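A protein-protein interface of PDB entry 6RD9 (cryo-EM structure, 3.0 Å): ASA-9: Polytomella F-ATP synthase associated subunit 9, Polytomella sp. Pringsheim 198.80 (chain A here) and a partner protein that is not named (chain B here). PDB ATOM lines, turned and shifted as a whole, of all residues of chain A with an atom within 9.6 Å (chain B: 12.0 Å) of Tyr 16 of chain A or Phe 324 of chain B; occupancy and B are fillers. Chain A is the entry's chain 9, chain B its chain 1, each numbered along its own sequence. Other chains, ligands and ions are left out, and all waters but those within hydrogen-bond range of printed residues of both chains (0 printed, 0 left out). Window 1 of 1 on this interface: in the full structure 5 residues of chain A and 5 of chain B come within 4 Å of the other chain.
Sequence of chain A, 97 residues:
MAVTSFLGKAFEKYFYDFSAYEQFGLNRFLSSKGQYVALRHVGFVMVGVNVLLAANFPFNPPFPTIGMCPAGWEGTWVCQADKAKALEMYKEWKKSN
Hydrophobic or aromatic side chains of chain A that line the printed part of chain B: Phe 11, Phe 15 and Tyr 16.
Among the printed residues, 10 pairs touch across the chains.
Tyr 16 of chain A touches just these residues of chain B: Phe 324, Leu 325, Leu 326, Lys 327 and Arg 328.
Phe 324 of chain B touches four residues of chain A.
Of chain B, only Phe 324 comes within 4 Å of Phe 11 of chain A.
Of chain B, only Phe 324 (3.7 Å) comes within 4 Å of Phe 15 of chain A.
No residue of chain B comes within 4 Å of Ser 19 of chain A.
Leu 325 of chain B touches just one residue of chain A: Tyr 16 (3.4 Å).
Of the printed residues of chain A, Arg 328 of chain B touches Tyr 16 and Asp 17.
Of the printed residues of chain A, Lys 327 of chain B touches Glu 12 (3.4 Å) and Tyr 16 (3.8 Å).
Printed residues of chain A within 4 Å of Leu 326 of chain B: Tyr 16 (3.96 Å).
Phe 18 of chain A touches none of the printed residues of chain B.
The nearest residue of chain A that does not touch Phe 324 of chain B is Gly 8 of chain A (4.9 Å).
The side-chain carboxylate (OE2) of Glu 12 of chain A lies within salt-bridge range of the side-chain amino group (NZ) of Lys 327 of chain B, at 3.4 Å.
The guanidinium group (NH2) of Arg 328 of chain B is in salt-bridge range of the side-chain carboxylate (OD2) of Asp 17 of chain A.
The backbone carbonyl oxygen (O) of Phe 324 of chain B lies close to the side-chain hydroxyl (OH) of Tyr 16 of chain A, 2.3 Å away.
Among the printed residues, pairs that only touch across the chains: Tyr 16 of chain A with Arg 328 of chain B (2.8 Å), Tyr 16 of chain A with Leu 325 of chain B (3.4 Å), Phe 11 of chain A with Phe 324 of chain B (3.4 Å), Phe 15 of chain A with Phe 324 of chain B (3.7 Å), Glu 12 of chain A with Phe 324 of chain B (3.7 Å), Tyr 16 of chain A with Lys 327 of chain B (3.8 Å) and Tyr 16 of chain A with Leu 326 of chain B (3.96 Å).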
ATOM      1  N   LEU A   7      16.920  10.931  28.007  1.00  0.00           N
ATOM      2  CA  LEU A   7      18.149  11.704  27.990  1.00  0.00           C
ATOM      3  C   LEU A   7      18.031  12.930  27.110  1.00  0.00           C
ATOM      4  O   LEU A   7      18.903  13.795  27.162  1.00  0.00           O
ATOM      5  CB  LEU A   7      19.346  10.839  27.579  1.00  0.00           C
ATOM      6  CG  LEU A   7      19.677  10.445  26.144  1.00  0.00           C
ATOM      7  CD1 LEU A   7      21.090   9.911  26.118  1.00  0.00           C
ATOM      8  CD2 LEU A   7      18.734   9.414  25.608  1.00  0.00           C
ATOM      9  N   GLY A   8      16.950  13.041  26.337  1.00  0.00           N
ATOM     10  CA  GLY A   8      16.590  14.332  25.787  1.00  0.00           C
ATOM     11  C   GLY A   8      16.260  15.329  26.877  1.00  0.00           C
ATOM     12  O   GLY A   8      16.631  16.499  26.791  1.00  0.00           O
ATOM     13  N   LYS A   9      15.589  14.870  27.936  1.00  0.00           N
ATOM     14  CA  LYS A   9      15.335  15.728  29.086  1.00  0.00           C
ATOM     15  C   LYS A   9      16.561  15.857  29.967  1.00  0.00           C
ATOM     16  O   LYS A   9      16.681  16.832  30.713  1.00  0.00           O
ATOM     17  CB  LYS A   9      14.164  15.199  29.909  1.00  0.00           C
ATOM     18  CG  LYS A   9      12.819  15.332  29.231  1.00  0.00           C
ATOM     19  CD  LYS A   9      11.678  15.212  30.231  1.00  0.00           C
ATOM     20  CE  LYS A   9      11.407  13.776  30.619  1.00  0.00           C
ATOM     21  NZ  LYS A   9      10.775  13.017  29.513  1.00  0.00           N
ATOM     22  N   ALA A  10      17.469  14.886  29.911  1.00  0.00           N
ATOM     23  CA  ALA A  10      18.716  15.027  30.645  1.00  0.00           C
ATOM     24  C   ALA A  10      19.672  15.962  29.930  1.00  0.00           C
ATOM     25  O   ALA A  10      20.342  16.776  30.576  1.00  0.00           O
ATOM     26  CB  ALA A  10      19.369  13.668  30.850  1.00  0.00           C
ATOM     27  N   PHE A  11      19.748  15.861  28.598  1.00  0.00           N
ATOM     28  CA  PHE A  11      20.581  16.784  27.840  1.00  0.00           C
ATOM     29  C   PHE A  11      20.018  18.191  27.877  1.00  0.00           C
ATOM     30  O   PHE A  11      20.784  19.154  27.847  1.00  0.00           O
ATOM     31  CB  PHE A  11      20.737  16.325  26.395  1.00  0.00           C
ATOM     32  CG  PHE A  11      21.516  17.277  25.554  1.00  0.00           C
ATOM     33  CD1 PHE A  11      22.854  17.486  25.799  1.00  0.00           C
ATOM     34  CD2 PHE A  11      20.910  17.992  24.546  1.00  0.00           C
ATOM     35  CE1 PHE A  11      23.570  18.373  25.047  1.00  0.00           C
ATOM     36  CE2 PHE A  11      21.631  18.872  23.795  1.00  0.00           C
ATOM     37  CZ  PHE A  11      22.957  19.067  24.052  1.00  0.00           C
ATOM     38  N   GLU A  12      18.695  18.327  27.981  1.00  0.00           N
ATOM     39  CA  GLU A  12      18.081  19.644  28.075  1.00  0.00           C
ATOM     40  C   GLU A  12      18.497  20.366  29.345  1.00  0.00           C
ATOM     41  O   GLU A  12      18.840  21.551  29.311  1.00  0.00           O
ATOM     42  CB  GLU A  12      16.567  19.518  28.021  1.00  0.00           C
ATOM     43  CG  GLU A  12      15.853  20.834  28.126  1.00  0.00           C
ATOM     44  CD  GLU A  12      14.421  20.669  28.519  1.00  0.00           C
ATOM     45  OE1 GLU A  12      13.982  21.380  29.440  1.00  0.00           O
ATOM     46  OE2 GLU A  12      13.736  19.821  27.915  1.00  0.00           O
ATOM     47  N   LYS A  13      18.490  19.671  30.474  1.00  0.00           N
ATOM     48  CA  LYS A  13      18.938  20.294  31.706  1.00  0.00           C
ATOM     49  C   LYS A  13      20.436  20.164  31.917  1.00  0.00           C
ATOM     50  O   LYS A  13      20.953  20.703  32.894  1.00  0.00           O
ATOM     51  CB  LYS A  13      18.168  19.738  32.909  1.00  0.00           C
ATOM     52  CG  LYS A  13      18.311  18.255  33.203  1.00  0.00           C
ATOM     53  CD  LYS A  13      17.457  17.910  34.439  1.00  0.00           C
ATOM     54  CE  LYS A  13      17.593  16.459  34.926  1.00  0.00           C
ATOM     55  NZ  LYS A  13      16.926  15.435  34.080  1.00  0.00           N
ATOM     56  N   TYR A  14      21.153  19.493  31.021  1.00  0.00           N
ATOM     57  CA  TYR A  14      22.589  19.715  30.973  1.00  0.00           C
ATOM     58  C   TYR A  14      22.931  20.905  30.082  1.00  0.00           C
ATOM     59  O   TYR A  14      23.878  21.645  30.366  1.00  0.00           O
ATOM     60  CB  TYR A  14      23.314  18.455  30.492  1.00  0.00           C
ATOM     61  CG  TYR A  14      24.718  18.732  30.029  1.00  0.00           C
ATOM     62  CD1 TYR A  14      25.704  19.122  30.921  1.00  0.00           C
ATOM     63  CD2 TYR A  14      25.049  18.642  28.691  1.00  0.00           C
ATOM     64  CE1 TYR A  14      26.974  19.407  30.493  1.00  0.00           C
ATOM     65  CE2 TYR A  14      26.314  18.921  28.257  1.00  0.00           C
ATOM     66  CZ  TYR A  14      27.269  19.301  29.159  1.00  0.00           C
ATOM     67  OH  TYR A  14      28.531  19.570  28.709  1.00  0.00           O
ATOM     68  N   PHE A  15      22.154  21.120  29.023  1.00  0.00           N
ATOM     69  CA  PHE A  15      22.421  22.229  28.117  1.00  0.00           C
ATOM     70  C   PHE A  15      22.107  23.563  28.768  1.00  0.00           C
ATOM     71  O   PHE A  15      22.886  24.510  28.659  1.00  0.00           O
ATOM     72  CB  PHE A  15      21.604  22.062  26.838  1.00  0.00           C
ATOM     73  CG  PHE A  15      21.965  23.013  25.754  1.00  0.00           C
ATOM     74  CD1 PHE A  15      21.234  24.161  25.550  1.00  0.00           C
ATOM     75  CD2 PHE A  15      23.021  22.753  24.923  1.00  0.00           C
ATOM     76  CE1 PHE A  15      21.567  25.038  24.566  1.00  0.00           C
ATOM     77  CE2 PHE A  15      23.348  23.630  23.933  1.00  0.00           C
ATOM     78  CZ  PHE A  15      22.620  24.772  23.756  1.00  0.00           C
ATOM     79  N   TYR A  16      20.986  23.653  29.469  1.00  0.00           N
ATOM     80  CA  TYR A  16      20.422  24.962  29.754  1.00  0.00           C
ATOM     81  C   TYR A  16      20.867  25.535  31.089  1.00  0.00           C
ATOM     82  O   TYR A  16      21.505  26.591  31.132  1.00  0.00           O
ATOM     83  CB  TYR A  16      18.903  24.883  29.693  1.00  0.00           C
ATOM     84  CG  TYR A  16      18.383  25.164  28.324  1.00  0.00           C
ATOM     85  CD1 TYR A  16      17.795  24.171  27.571  1.00  0.00           C
ATOM     86  CD2 TYR A  16      18.502  26.421  27.778  1.00  0.00           C
ATOM     87  CE1 TYR A  16      17.335  24.427  26.325  1.00  0.00           C
ATOM     88  CE2 TYR A  16      18.049  26.681  26.536  1.00  0.00           C
ATOM     89  CZ  TYR A  16      17.466  25.683  25.814  1.00  0.00           C
ATOM     90  OH  TYR A  16      17.009  25.961  24.562  1.00  0.00           O
ATOM     91  N   ASP A  17      20.545  24.855  32.182  1.00  0.00           N
ATOM     92  CA  ASP A  17      20.766  25.421  33.502  1.00  0.00           C
ATOM     93  C   ASP A  17      21.980  24.846  34.211  1.00  0.00           C
ATOM     94  O   ASP A  17      22.486  25.484  35.138  1.00  0.00           O
ATOM     95  CB  ASP A  17      19.510  25.240  34.359  1.00  0.00           C
ATOM     96  CG  ASP A  17      18.927  23.865  34.232  1.00  0.00           C
ATOM     97  OD1 ASP A  17      19.533  23.042  33.529  1.00  0.00           O
ATOM     98  OD2 ASP A  17      17.845  23.618  34.794  1.00  0.00           O
ATOM     99  N   PHE A  18      22.458  23.676  33.800  1.00  0.00           N
ATOM    100  CA  PHE A  18      23.772  23.196  34.216  1.00  0.00           C
ATOM    101  C   PHE A  18      24.797  24.155  33.650  1.00  0.00           C
ATOM    102  O   PHE A  18      25.063  24.155  32.451  1.00  0.00           O
ATOM    103  CB  PHE A  18      24.023  21.788  33.696  1.00  0.00           C
ATOM    104  CG  PHE A  18      25.091  21.031  34.440  1.00  0.00           C
ATOM    105  CD1 PHE A  18      26.436  21.358  34.301  1.00  0.00           C
ATOM    106  CD2 PHE A  18      24.750  19.944  35.229  1.00  0.00           C
ATOM    107  CE1 PHE A  18      27.404  20.657  34.973  1.00  0.00           C
ATOM    108  CE2 PHE A  18      25.715  19.231  35.901  1.00  0.00           C
ATOM    109  CZ  PHE A  18      27.044  19.586  35.770  1.00  0.00           C
ATOM    110  N   SER A  19      25.381  24.984  34.500  1.00  0.00           N
ATOM    111  CA  SER A  19      26.370  25.950  34.055  1.00  0.00           C
ATOM    112  C   SER A  19      27.536  25.933  35.017  1.00  0.00           C
ATOM    113  O   SER A  19      27.406  26.384  36.156  1.00  0.00           O
ATOM    114  CB  SER A  19      25.774  27.350  33.973  1.00  0.00           C
ATOM    115  OG  SER A  19      26.765  28.291  33.615  1.00  0.00           O
ATOM    116  N   ALA A  20      28.686  25.464  34.551  1.00  0.00           N
ATOM    117  CA  ALA A  20      29.891  25.523  35.357  1.00  0.00           C
ATOM    118  C   ALA A  20      30.501  26.909  35.405  1.00  0.00           C
ATOM    119  O   ALA A  20      31.515  27.088  36.076  1.00  0.00           O
ATOM    120  CB  ALA A  20      30.927  24.530  34.843  1.00  0.00           C
ATOM    121  N   TYR A  21      29.941  27.890  34.706  1.00  0.00           N
ATOM    122  CA  TYR A  21      30.425  29.248  34.870  1.00  0.00           C
ATOM    123  C   TYR A  21      29.949  29.860  36.169  1.00  0.00           C
ATOM    124  O   TYR A  21      30.596  30.772  36.683  1.00  0.00           O
ATOM    125  CB  TYR A  21      29.982  30.116  33.705  1.00  0.00           C
ATOM    126  CG  TYR A  21      30.449  31.540  33.796  1.00  0.00           C
ATOM    127  CD1 TYR A  21      31.786  31.851  33.716  1.00  0.00           C
ATOM    128  CD2 TYR A  21      29.550  32.568  33.984  1.00  0.00           C
ATOM    129  CE1 TYR A  21      32.215  33.147  33.793  1.00  0.00           C
ATOM    130  CE2 TYR A  21      29.966  33.867  34.065  1.00  0.00           C
ATOM    131  CZ  TYR A  21      31.300  34.150  33.971  1.00  0.00           C
ATOM    132  OH  TYR A  21      31.726  35.451  34.051  1.00  0.00           O
ATOM    133  N   GLU A  22      28.842  29.384  36.712  1.00  0.00           N
ATOM    134  CA  GLU A  22      28.353  29.866  37.991  1.00  0.00           C
ATOM    135  C   GLU A  22      28.350  28.812  39.082  1.00  0.00           C
ATOM    136  O   GLU A  22      28.555  29.161  40.241  1.00  0.00           O
ATOM    137  CB  GLU A  22      26.944  30.461  37.832  1.00  0.00           C
ATOM    138  CG  GLU A  22      25.932  29.567  37.119  1.00  0.00           C
ATOM    139  CD  GLU A  22      25.200  28.603  38.037  1.00  0.00           C
ATOM    140  OE1 GLU A  22      25.188  28.825  39.265  1.00  0.00           O
ATOM    141  OE2 GLU A  22      24.630  27.619  37.527  1.00  0.00           O
ATOM    142  N   LYS A  33      30.946  36.462  30.506  1.00  0.00           N
ATOM    143  CA  LYS A  33      30.750  35.091  30.060  1.00  0.00           C
ATOM    144  C   LYS A  33      31.132  34.905  28.605  1.00  0.00           C
ATOM    145  O   LYS A  33      31.371  33.775  28.178  1.00  0.00           O
ATOM    146  CB  LYS A  33      29.302  34.637  30.259  1.00  0.00           C
ATOM    147  CG  LYS A  33      29.194  33.146  30.458  1.00  0.00           C
ATOM    148  CD  LYS A  33      27.781  32.652  30.527  1.00  0.00           C
ATOM    149  CE  LYS A  33      27.787  31.142  30.687  1.00  0.00           C
ATOM    150  NZ  LYS A  33      26.419  30.567  30.752  1.00  0.00           N
ATOM    151  N   LEU B 315       2.457  33.021  20.100  1.00  0.00           N
ATOM    152  CA  LEU B 315       3.750  32.540  19.650  1.00  0.00           C
ATOM    153  C   LEU B 315       4.434  31.655  20.665  1.00  0.00           C
ATOM    154  O   LEU B 315       5.271  30.853  20.288  1.00  0.00           O
ATOM    155  CB  LEU B 315       4.680  33.699  19.343  1.00  0.00           C
ATOM    156  CG  LEU B 315       4.809  34.190  17.919  1.00  0.00           C
ATOM    157  CD1 LEU B 315       5.860  35.228  17.907  1.00  0.00           C
ATOM    158  CD2 LEU B 315       5.195  33.076  17.021  1.00  0.00           C
ATOM    159  N   ASN B 316       4.137  31.803  21.945  1.00  0.00           N
ATOM    160  CA  ASN B 316       4.799  30.987  22.947  1.00  0.00           C
ATOM    161  C   ASN B 316       4.307  29.561  22.922  1.00  0.00           C
ATOM    162  O   ASN B 316       5.041  28.646  23.295  1.00  0.00           O
ATOM    163  CB  ASN B 316       4.561  31.570  24.316  1.00  0.00           C
ATOM    164  CG  ASN B 316       5.504  32.643  24.628  1.00  0.00           C
ATOM    165  OD1 ASN B 316       5.135  33.685  25.140  1.00  0.00           O
ATOM    166  ND2 ASN B 316       6.751  32.403  24.332  1.00  0.00           N
ATOM    167  N   SER B 318       3.369  28.217  20.101  1.00  0.00           N
ATOM    168  CA  SER B 318       3.660  27.779  18.753  1.00  0.00           C
ATOM    169  C   SER B 318       4.545  26.545  18.803  1.00  0.00           C
ATOM    170  O   SER B 318       5.193  26.286  19.815  1.00  0.00           O
ATOM    171  CB  SER B 318       4.371  28.891  18.000  1.00  0.00           C
ATOM    172  OG  SER B 318       4.406  28.684  16.613  1.00  0.00           O
ATOM    173  N   PRO B 319       4.600  25.765  17.722  1.00  0.00           N
ATOM    174  CA  PRO B 319       5.587  24.685  17.663  1.00  0.00           C
ATOM    175  C   PRO B 319       7.019  25.160  17.626  1.00  0.00           C
ATOM    176  O   PRO B 319       7.920  24.353  17.839  1.00  0.00           O
ATOM    177  CB  PRO B 319       5.213  23.953  16.379  1.00  0.00           C
ATOM    178  CG  PRO B 319       3.823  24.222  16.201  1.00  0.00           C
ATOM    179  CD  PRO B 319       3.563  25.579  16.699  1.00  0.00           C
ATOM    180  N   ALA B 320       7.265  26.433  17.356  1.00  0.00           N
ATOM    181  CA  ALA B 320       8.627  26.925  17.285  1.00  0.00           C
ATOM    182  C   ALA B 320       9.257  27.054  18.645  1.00  0.00           C
ATOM    183  O   ALA B 320      10.474  26.954  18.764  1.00  0.00           O
ATOM    184  CB  ALA B 320       8.652  28.277  16.609  1.00  0.00           C
ATOM    185  N   PHE B 321       8.468  27.315  19.670  1.00  0.00           N
ATOM    186  CA  PHE B 321       9.004  27.625  20.981  1.00  0.00           C
ATOM    187  C   PHE B 321       9.031  26.418  21.886  1.00  0.00           C
ATOM    188  O   PHE B 321       9.521  26.506  23.005  1.00  0.00           O
ATOM    189  CB  PHE B 321       8.211  28.761  21.605  1.00  0.00           C
ATOM    190  CG  PHE B 321       8.663  30.096  21.156  1.00  0.00           C
ATOM    191  CD1 PHE B 321       9.454  30.874  21.952  1.00  0.00           C
ATOM    192  CD2 PHE B 321       8.339  30.553  19.916  1.00  0.00           C
ATOM    193  CE1 PHE B 321       9.893  32.082  21.516  1.00  0.00           C
ATOM    194  CE2 PHE B 321       8.767  31.755  19.491  1.00  0.00           C
ATOM    195  CZ  PHE B 321       9.551  32.517  20.291  1.00  0.00           C
ATOM    196  N   SER B 322       8.513  25.300  21.429  1.00  0.00           N
ATOM    197  CA  SER B 322       8.752  24.022  22.058  1.00  0.00           C
ATOM    198  C   SER B 322       9.955  23.321  21.464  1.00  0.00           C
ATOM    199  O   SER B 322      10.240  22.187  21.843  1.00  0.00           O
ATOM    200  CB  SER B 322       7.536  23.127  21.912  1.00  0.00           C
ATOM    201  OG  SER B 322       7.403  22.716  20.569  1.00  0.00           O
ATOM    202  N   SER B 323      10.636  23.947  20.513  1.00  0.00           N
ATOM    203  CA  SER B 323      11.867  23.404  19.986  1.00  0.00           C
ATOM    204  C   SER B 323      12.970  23.567  21.005  1.00  0.00           C
ATOM    205  O   SER B 323      12.847  24.326  21.961  1.00  0.00           O
ATOM    206  CB  SER B 323      12.248  24.092  18.691  1.00  0.00           C
ATOM    207  OG  SER B 323      11.327  23.766  17.682  1.00  0.00           O
ATOM    208  N   PHE B 324      14.072  22.860  20.773  1.00  0.00           N
ATOM    209  CA  PHE B 324      15.115  22.757  21.778  1.00  0.00           C
ATOM    210  C   PHE B 324      15.817  24.085  22.001  1.00  0.00           C
ATOM    211  O   PHE B 324      16.057  24.479  23.139  1.00  0.00           O
ATOM    212  CB  PHE B 324      16.124  21.691  21.379  1.00  0.00           C
ATOM    213  CG  PHE B 324      17.199  21.496  22.389  1.00  0.00           C
ATOM    214  CD1 PHE B 324      16.943  20.803  23.545  1.00  0.00           C
ATOM    215  CD2 PHE B 324      18.452  22.033  22.203  1.00  0.00           C
ATOM    216  CE1 PHE B 324      17.905  20.646  24.474  1.00  0.00           C
ATOM    217  CE2 PHE B 324      19.404  21.881  23.140  1.00  0.00           C
ATOM    218  CZ  PHE B 324      19.130  21.189  24.274  1.00  0.00           C
ATOM    219  N   LEU B 325      16.160  24.784  20.939  1.00  0.00           N
ATOM    220  CA  LEU B 325      16.910  26.019  21.090  1.00  0.00           C
ATOM    221  C   LEU B 325      16.050  27.193  21.508  1.00  0.00           C
ATOM    222  O   LEU B 325      16.592  28.255  21.812  1.00  0.00           O
ATOM    223  CB  LEU B 325      17.613  26.354  19.789  1.00  0.00           C
ATOM    224  CG  LEU B 325      18.630  25.314  19.374  1.00  0.00           C
ATOM    225  CD1 LEU B 325      19.012  25.556  17.958  1.00  0.00           C
ATOM    226  CD2 LEU B 325      19.828  25.428  20.268  1.00  0.00           C
ATOM    227  N   LEU B 326      14.734  27.041  21.509  1.00  0.00           N
ATOM    228  CA  LEU B 326      13.835  28.112  21.901  1.00  0.00           C
ATOM    229  C   LEU B 326      12.974  27.716  23.079  1.00  0.00           C
ATOM    230  O   LEU B 326      11.955  28.352  23.324  1.00  0.00           O
ATOM    231  CB  LEU B 326      12.940  28.519  20.736  1.00  0.00           C
ATOM    232  CG  LEU B 326      13.551  29.293  19.588  1.00  0.00           C
ATOM    233  CD1 LEU B 326      12.485  29.570  18.619  1.00  0.00           C
ATOM    234  CD2 LEU B 326      14.102  30.559  20.112  1.00  0.00           C
ATOM    235  N   LYS B 327      13.375  26.689  23.823  1.00  0.00           N
ATOM    236  CA  LYS B 327      12.491  26.101  24.820  1.00  0.00           C
ATOM    237  C   LYS B 327      12.358  26.985  26.050  1.00  0.00           C
ATOM    238  O   LYS B 327      11.266  27.115  26.606  1.00  0.00           O
ATOM    239  CB  LYS B 327      12.997  24.725  25.210  1.00  0.00           C
ATOM    240  CG  LYS B 327      11.915  23.822  25.663  1.00  0.00           C
ATOM    241  CD  LYS B 327      12.410  22.417  25.818  1.00  0.00           C
ATOM    242  CE  LYS B 327      12.645  21.788  24.492  1.00  0.00           C
ATOM    243  NZ  LYS B 327      13.034  20.373  24.608  1.00  0.00           N
ATOM    244  N   ARG B 328      13.471  27.604  26.451  1.00  0.00           N
ATOM    245  CA  ARG B 328      13.487  28.495  27.642  1.00  0.00           C
ATOM    246  C   ARG B 328      13.349  29.956  27.199  1.00  0.00           C
ATOM    247  O   ARG B 328      13.773  30.844  27.965  1.00  0.00           O
ATOM    248  CB  ARG B 328      14.773  28.284  28.448  1.00  0.00           C
ATOM    249  CG  ARG B 328      14.888  26.906  29.085  1.00  0.00           C
ATOM    250  CD  ARG B 328      16.140  26.763  29.932  1.00  0.00           C
ATOM    251  NE  ARG B 328      16.260  25.437  30.521  1.00  0.00           N
ATOM    252  CZ  ARG B 328      15.656  25.053  31.640  1.00  0.00           C
ATOM    253  NH1 ARG B 328      14.881  25.898  32.298  1.00  0.00           N
ATOM    254  NH2 ARG B 328      15.829  23.826  32.096  1.00  0.00           N
ATOM    255  N   GLU B 329      12.781  30.194  26.011  1.00  0.00           N
ATOM    256  CA  GLU B 329      12.608  31.549  25.525  1.00  0.00           C
ATOM    257  C   GLU B 329      11.151  31.967  25.594  1.00  0.00           C
ATOM    258  O   GLU B 329      10.239  31.142  25.635  1.00  0.00           O
ATOM    259  CB  GLU B 329      13.108  31.681  24.093  1.00  0.00           C
ATOM    260  CG  GLU B 329      14.591  31.785  23.979  1.00  0.00           C
ATOM    261  CD  GLU B 329      15.158  32.840  24.882  1.00  0.00           C
ATOM    262  OE1 GLU B 329      16.090  32.518  25.643  1.00  0.00           O
ATOM    263  OE2 GLU B 329      14.677  33.991  24.842  1.00  0.00           O
ATOM    264  N   LYS B 330      10.946  33.270  25.599  1.00  0.00           N
ATOM    265  CA  LYS B 330       9.616  33.837  25.614  1.00  0.00           C
ATOM    266  C   LYS B 330       9.510  34.850  24.492  1.00  0.00           C
ATOM    267  O   LYS B 330      10.436  35.624  24.260  1.00  0.00           O
ATOM    268  CB  LYS B 330       9.315  34.483  26.960  1.00  0.00           C
ATOM    269  CG  LYS B 330       9.118  33.481  28.076  1.00  0.00           C
ATOM    270  CD  LYS B 330       8.025  32.502  27.720  1.00  0.00           C
ATOM    271  CE  LYS B 330       8.194  31.187  28.439  1.00  0.00           C
ATOM    272  NZ  LYS B 330       7.157  30.216  27.997  1.00  0.00           N
